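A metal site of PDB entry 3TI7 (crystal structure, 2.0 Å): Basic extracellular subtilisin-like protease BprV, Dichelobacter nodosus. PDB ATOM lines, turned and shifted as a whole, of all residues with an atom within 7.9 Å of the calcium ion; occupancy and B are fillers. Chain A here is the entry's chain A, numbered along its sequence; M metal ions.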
ATOM      1  N   PRO A   3       8.667  27.378   4.412  1.00  0.00           N
ATOM      2  CA  PRO A   3       8.953  26.550   5.597  1.00  0.00           C
ATOM      3  C   PRO A   3      10.415  26.710   6.042  1.00  0.00           C
ATOM      4  O   PRO A   3      11.276  26.978   5.202  1.00  0.00           O
ATOM      5  CB  PRO A   3       8.701  25.122   5.103  1.00  0.00           C
ATOM      6  CG  PRO A   3       8.777  25.191   3.617  1.00  0.00           C
ATOM      7  CD  PRO A   3       8.283  26.561   3.242  1.00  0.00           C
ATOM      8  N   ASN A   4      10.656  26.550   7.349  1.00  0.00           N
ATOM      9  CA  ASN A   4      11.962  26.857   7.941  1.00  0.00           C
ATOM     10  C   ASN A   4      12.973  25.705   7.906  1.00  0.00           C
ATOM     11  O   ASN A   4      14.062  25.805   8.476  1.00  0.00           O
ATOM     12  CB  ASN A   4      11.789  27.383   9.382  1.00  0.00           C
ATOM     13  CG  ASN A   4      11.349  26.298  10.373  1.00  0.00           C
ATOM     14  OD1 ASN A   4      11.315  25.108  10.047  1.00  0.00           O
ATOM     15  ND2 ASN A   4      11.031  26.720  11.586  1.00  0.00           N
ATOM     16  N   ASP A   5      12.609  24.618   7.235  1.00  0.00           N
ATOM     17  CA  ASP A   5      13.475  23.448   7.164  1.00  0.00           C
ATOM     18  C   ASP A   5      14.757  23.830   6.425  1.00  0.00           C
ATOM     19  O   ASP A   5      14.690  24.336   5.305  1.00  0.00           O
ATOM     20  CB  ASP A   5      12.735  22.324   6.435  1.00  0.00           C
ATOM     21  CG  ASP A   5      11.364  22.070   7.021  1.00  0.00           C
ATOM     22  OD1 ASP A   5      11.247  21.166   7.878  1.00  0.00           O
ATOM     23  OD2 ASP A   5      10.409  22.783   6.641  1.00  0.00           O
ATOM     24  N   PRO A   6      15.931  23.596   7.057  1.00  0.00           N
ATOM     25  CA  PRO A   6      17.221  24.066   6.531  1.00  0.00           C
ATOM     26  C   PRO A   6      17.551  23.602   5.112  1.00  0.00           C
ATOM     27  O   PRO A   6      18.270  24.314   4.398  1.00  0.00           O
ATOM     28  CB  PRO A   6      18.255  23.525   7.543  1.00  0.00           C
ATOM     29  CG  PRO A   6      17.543  22.521   8.367  1.00  0.00           C
ATOM     30  CD  PRO A   6      16.091  22.876   8.343  1.00  0.00           C
ATOM     31  N   SER A   7      17.046  22.440   4.698  1.00  0.00           N
ATOM     32  CA  SER A   7      17.320  21.905   3.355  1.00  0.00           C
ATOM     33  C   SER A   7      16.203  22.158   2.347  1.00  0.00           C
ATOM     34  O   SER A   7      16.330  21.754   1.188  1.00  0.00           O
ATOM     35  CB  SER A   7      17.667  20.415   3.399  1.00  0.00           C
ATOM     36  OG  SER A   7      18.931  20.210   4.028  1.00  0.00           O
ATOM     37  N   TYR A   8      15.116  22.802   2.757  1.00  0.00           N
ATOM     38  CA  TYR A   8      14.031  23.145   1.827  1.00  0.00           C
ATOM     39  C   TYR A   8      14.543  23.972   0.631  1.00  0.00           C
ATOM     40  O   TYR A   8      14.126  23.748  -0.513  1.00  0.00           O
ATOM     41  CB  TYR A   8      12.874  23.883   2.521  1.00  0.00           C
ATOM     42  CG  TYR A   8      11.928  24.550   1.559  1.00  0.00           C
ATOM     43  CD1 TYR A   8      11.072  23.796   0.752  1.00  0.00           C
ATOM     44  CD2 TYR A   8      11.889  25.947   1.425  1.00  0.00           C
ATOM     45  CE1 TYR A   8      10.200  24.397  -0.144  1.00  0.00           C
ATOM     46  CE2 TYR A   8      11.024  26.561   0.530  1.00  0.00           C
ATOM     47  CZ  TYR A   8      10.182  25.797  -0.252  1.00  0.00           C
ATOM     48  OH  TYR A   8       9.325  26.390  -1.148  1.00  0.00           O
ATOM     49  N   GLN A  11      15.398  22.065  -2.309  1.00  0.00           N
ATOM     50  CA  GLN A  11      14.319  21.299  -2.946  1.00  0.00           C
ATOM     51  C   GLN A  11      13.656  22.090  -4.078  1.00  0.00           C
ATOM     52  O   GLN A  11      12.456  22.375  -4.054  1.00  0.00           O
ATOM     53  CB  GLN A  11      13.321  20.793  -1.906  1.00  0.00           C
ATOM     54  CG  GLN A  11      13.928  19.765  -0.910  1.00  0.00           C
ATOM     55  CD  GLN A  11      12.938  19.319   0.149  1.00  0.00           C
ATOM     56  OE1 GLN A  11      12.471  20.104   0.971  1.00  0.00           O
ATOM     57  NE2 GLN A  11      12.608  18.043   0.137  1.00  0.00           N
ATOM     58  N   HIS A  47      12.643   7.864  11.711  1.00  0.00           N
ATOM     59  CA  HIS A  47      13.294   9.070  11.209  1.00  0.00           C
ATOM     60  C   HIS A  47      12.578  10.279  11.820  1.00  0.00           C
ATOM     61  O   HIS A  47      11.356  10.409  11.672  1.00  0.00           O
ATOM     62  CB  HIS A  47      13.190   9.083   9.679  1.00  0.00           C
ATOM     63  CG  HIS A  47      14.131  10.025   8.993  1.00  0.00           C
ATOM     64  ND1 HIS A  47      14.187  11.377   9.275  1.00  0.00           N
ATOM     65  CD2 HIS A  47      15.044   9.820   8.008  1.00  0.00           C
ATOM     66  CE1 HIS A  47      15.097  11.957   8.509  1.00  0.00           C
ATOM     67  NE2 HIS A  47      15.625  11.026   7.728  1.00  0.00           N
ATOM     68  N   VAL A  48      13.333  11.134  12.504  1.00  0.00           N
ATOM     69  CA  VAL A  48      12.811  12.377  13.117  1.00  0.00           C
ATOM     70  C   VAL A  48      11.967  13.229  12.159  1.00  0.00           C
ATOM     71  O   VAL A  48      10.974  13.842  12.576  1.00  0.00           O
ATOM     72  CB  VAL A  48      13.965  13.224  13.732  1.00  0.00           C
ATOM     73  CG1 VAL A  48      14.938  13.722  12.654  1.00  0.00           C
ATOM     74  CG2 VAL A  48      13.415  14.392  14.572  1.00  0.00           C
ATOM     75  N   ASP A  49      12.349  13.267  10.889  1.00  0.00           N
ATOM     76  CA  ASP A  49      11.641  14.065   9.906  1.00  0.00           C
ATOM     77  C   ASP A  49      10.521  13.296   9.194  1.00  0.00           C
ATOM     78  O   ASP A  49       9.960  13.777   8.219  1.00  0.00           O
ATOM     79  CB  ASP A  49      12.610  14.660   8.882  1.00  0.00           C
ATOM     80  CG  ASP A  49      12.360  16.140   8.645  1.00  0.00           C
ATOM     81  OD1 ASP A  49      11.788  16.783   9.555  1.00  0.00           O
ATOM     82  OD2 ASP A  49      12.739  16.675   7.577  1.00  0.00           O
ATOM     83  N   LEU A  50      10.217  12.100   9.686  1.00  0.00           N
ATOM     84  CA  LEU A  50       9.111  11.303   9.125  1.00  0.00           C
ATOM     85  C   LEU A  50       8.041  10.899  10.137  1.00  0.00           C
ATOM     86  O   LEU A  50       6.856  10.929   9.819  1.00  0.00           O
ATOM     87  CB  LEU A  50       9.624  10.040   8.413  1.00  0.00           C
ATOM     88  CG  LEU A  50      10.346  10.186   7.067  1.00  0.00           C
ATOM     89  CD1 LEU A  50      10.772   8.804   6.563  1.00  0.00           C
ATOM     90  CD2 LEU A  50       9.436  10.869   6.042  1.00  0.00           C
ATOM     91  N   ALA A 115       7.145  14.595   4.515  1.00  0.00           N
ATOM     92  CA  ALA A 115       8.191  14.871   5.508  1.00  0.00           C
ATOM     93  C   ALA A 115       7.657  15.932   6.455  1.00  0.00           C
ATOM     94  O   ALA A 115       6.910  16.837   6.037  1.00  0.00           O
ATOM     95  CB  ALA A 115       9.482  15.359   4.832  1.00  0.00           C
ATOM     96  N   VAL A 116       8.008  15.808   7.728  1.00  0.00           N
ATOM     97  CA  VAL A 116       7.596  16.793   8.734  1.00  0.00           C
ATOM     98  C   VAL A 116       8.250  18.120   8.352  1.00  0.00           C
ATOM     99  O   VAL A 116       9.476  18.206   8.207  1.00  0.00           O
ATOM    100  CB  VAL A 116       7.979  16.375  10.175  1.00  0.00           C
ATOM    101  CG1 VAL A 116       7.515  17.432  11.178  1.00  0.00           C
ATOM    102  CG2 VAL A 116       7.355  15.008  10.535  1.00  0.00           C
ATOM    103  N   THR A 117       7.404  19.125   8.175  1.00  0.00           N
ATOM    104  CA  THR A 117       7.787  20.373   7.562  1.00  0.00           C
ATOM    105  C   THR A 117       7.592  21.510   8.567  1.00  0.00           C
ATOM    106  O   THR A 117       6.774  21.408   9.498  1.00  0.00           O
ATOM    107  CB  THR A 117       6.956  20.591   6.294  1.00  0.00           C
ATOM    108  OG1 THR A 117       7.177  19.479   5.405  1.00  0.00           O
ATOM    109  CG2 THR A 117       7.316  21.876   5.574  1.00  0.00           C
ATOM    110  N   ASN A 118       8.357  22.585   8.387  1.00  0.00           N
ATOM    111  CA  ASN A 118       8.382  23.731   9.296  1.00  0.00           C
ATOM    112  C   ASN A 118       8.725  23.313  10.723  1.00  0.00           C
ATOM    113  O   ASN A 118       8.186  23.866  11.687  1.00  0.00           O
ATOM    114  CB  ASN A 118       7.063  24.538   9.209  1.00  0.00           C
ATOM    115  CG  ASN A 118       7.254  26.027   9.469  1.00  0.00           C
ATOM    116  OD1 ASN A 118       8.357  26.579   8.985  1.00  0.00           O
ATOM    117  ND2 ASN A 118       6.414  26.665  10.114  1.00  0.00           N
ATOM    118  N   ASN A 119       9.625  22.330  10.854  1.00  0.00           N
ATOM    119  CA  ASN A 119      10.078  21.823  12.158  1.00  0.00           C
ATOM    120  C   ASN A 119      11.571  22.066  12.449  1.00  0.00           C
ATOM    121  O   ASN A 119      12.146  21.449  13.360  1.00  0.00           O
ATOM    122  CB  ASN A 119       9.700  20.337  12.368  1.00  0.00           C
ATOM    123  CG  ASN A 119      10.541  19.376  11.508  1.00  0.00           C
ATOM    124  OD1 ASN A 119      11.104  19.760  10.470  1.00  0.00           O
ATOM    125  ND2 ASN A 119      10.600  18.112  11.927  1.00  0.00           N
ATOM    126  N   GLY A 120      12.175  22.957  11.677  1.00  0.00           N
ATOM    127  CA  GLY A 120      13.540  23.436  11.903  1.00  0.00           C
ATOM    128  C   GLY A 120      14.621  22.408  11.623  1.00  0.00           C
ATOM    129  O   GLY A 120      15.767  22.601  12.027  1.00  0.00           O
ATOM    130  N   VAL A 121      14.272  21.323  10.932  1.00  0.00           N
ATOM    131  CA  VAL A 121      15.236  20.246  10.685  1.00  0.00           C
ATOM    132  C   VAL A 121      14.916  19.524   9.371  1.00  0.00           C
ATOM    133  O   VAL A 121      13.751  19.347   9.019  1.00  0.00           O
ATOM    134  CB  VAL A 121      15.380  19.260  11.910  1.00  0.00           C
ATOM    135  CG1 VAL A 121      14.062  18.557  12.260  1.00  0.00           C
ATOM    136  CG2 VAL A 121      16.496  18.248  11.701  1.00  0.00           C
ATOM    137  N   GLY A 122      15.961  19.141   8.652  1.00  0.00           N
ATOM    138  CA  GLY A 122      15.832  18.392   7.414  1.00  0.00           C
ATOM    139  C   GLY A 122      15.129  19.116   6.289  1.00  0.00           C
ATOM    140  O   GLY A 122      15.497  20.241   5.914  1.00  0.00           O
ATOM    141  N   VAL A 123      14.082  18.453   5.773  1.00  0.00           N
ATOM    142  CA  VAL A 123      13.435  18.825   4.511  1.00  0.00           C
ATOM    143  C   VAL A 123      11.937  19.096   4.661  1.00  0.00           C
ATOM    144  O   VAL A 123      11.372  18.949   5.748  1.00  0.00           O
ATOM    145  CB  VAL A 123      13.623  17.697   3.440  1.00  0.00           C
ATOM    146  CG1 VAL A 123      15.105  17.552   3.033  1.00  0.00           C
ATOM    147  CG2 VAL A 123      13.030  16.351   3.926  1.00  0.00           C
ATOM    148  N   ALA A 124      11.302  19.482   3.557  1.00  0.00           N
ATOM    149  CA  ALA A 124       9.847  19.628   3.498  1.00  0.00           C
ATOM    150  C   ALA A 124       9.234  18.511   2.665  1.00  0.00           C
ATOM    151  O   ALA A 124       9.942  17.808   1.946  1.00  0.00           O
ATOM    152  CB  ALA A 124       9.489  20.983   2.908  1.00  0.00           C
ATOM    153  N   GLY A 125       7.909  18.347   2.773  1.00  0.00           N
ATOM    154  CA  GLY A 125       7.150  17.415   1.926  1.00  0.00           C
ATOM    155  C   GLY A 125       6.068  18.187   1.180  1.00  0.00           C
ATOM    156  O   GLY A 125       5.627  19.236   1.643  1.00  0.00           O
ATOM    157  N   THR A 257      14.213  12.212   2.614  1.00  0.00           N
ATOM    158  CA  THR A 257      14.626  11.497   3.822  1.00  0.00           C
ATOM    159  C   THR A 257      15.162  10.082   3.558  1.00  0.00           C
ATOM    160  O   THR A 257      14.519   9.292   2.873  1.00  0.00           O
ATOM    161  CB  THR A 257      13.433  11.374   4.797  1.00  0.00           C
ATOM    162  OG1 THR A 257      12.256  11.043   4.049  1.00  0.00           O
ATOM    163  CG2 THR A 257      13.196  12.695   5.535  1.00  0.00           C
ATOM    164  N   TYR A 270      19.540  12.799   4.946  1.00  0.00           N
ATOM    165  CA  TYR A 270      18.843  13.372   3.806  1.00  0.00           C
ATOM    166  C   TYR A 270      19.759  13.237   2.615  1.00  0.00           C
ATOM    167  O   TYR A 270      20.972  13.410   2.743  1.00  0.00           O
ATOM    168  CB  TYR A 270      18.473  14.844   4.084  1.00  0.00           C
ATOM    169  CG  TYR A 270      17.841  15.021   5.448  1.00  0.00           C
ATOM    170  CD1 TYR A 270      16.462  14.859   5.624  1.00  0.00           C
ATOM    171  CD2 TYR A 270      18.632  15.265   6.572  1.00  0.00           C
ATOM    172  CE1 TYR A 270      15.876  14.976   6.877  1.00  0.00           C
ATOM    173  CE2 TYR A 270      18.064  15.379   7.838  1.00  0.00           C
ATOM    174  CZ  TYR A 270      16.690  15.224   7.978  1.00  0.00           C
ATOM    175  OH  TYR A 270      16.128  15.335   9.228  1.00  0.00           O
HETATM  176 CA    CA M   1      11.581  18.922   8.222  1.00  0.00          CA
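OD2 of Asp 5 lies within hydrogen-bond range of N of Asn 118, at 2.7 Å. The backbone NH of Asn 119 is in hydrogen-bond range of the side-chain amide oxygen of Asn 4 (3.4 Å). The backbone NH (N) of Asp 49 sits at hydrogen-bond distance from a ring nitrogen (ND1) of His 47.
The calcium ion is bound by the backbone carbonyl oxygen (O) of Val 116, the side-chain carboxylate (OD1) of Asp 5, the backbone carbonyl oxygen (O) of Val 121, the side-chain amide oxygen (OD1) of Asn 119, the backbone carbonyl oxygen (O) of Val 123, the side-chain carboxylate (OD1) of Asp 49 and the side-chain carboxylate (OD2) of Asp 49. The calcium ion has seven donor atoms within binding distance.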
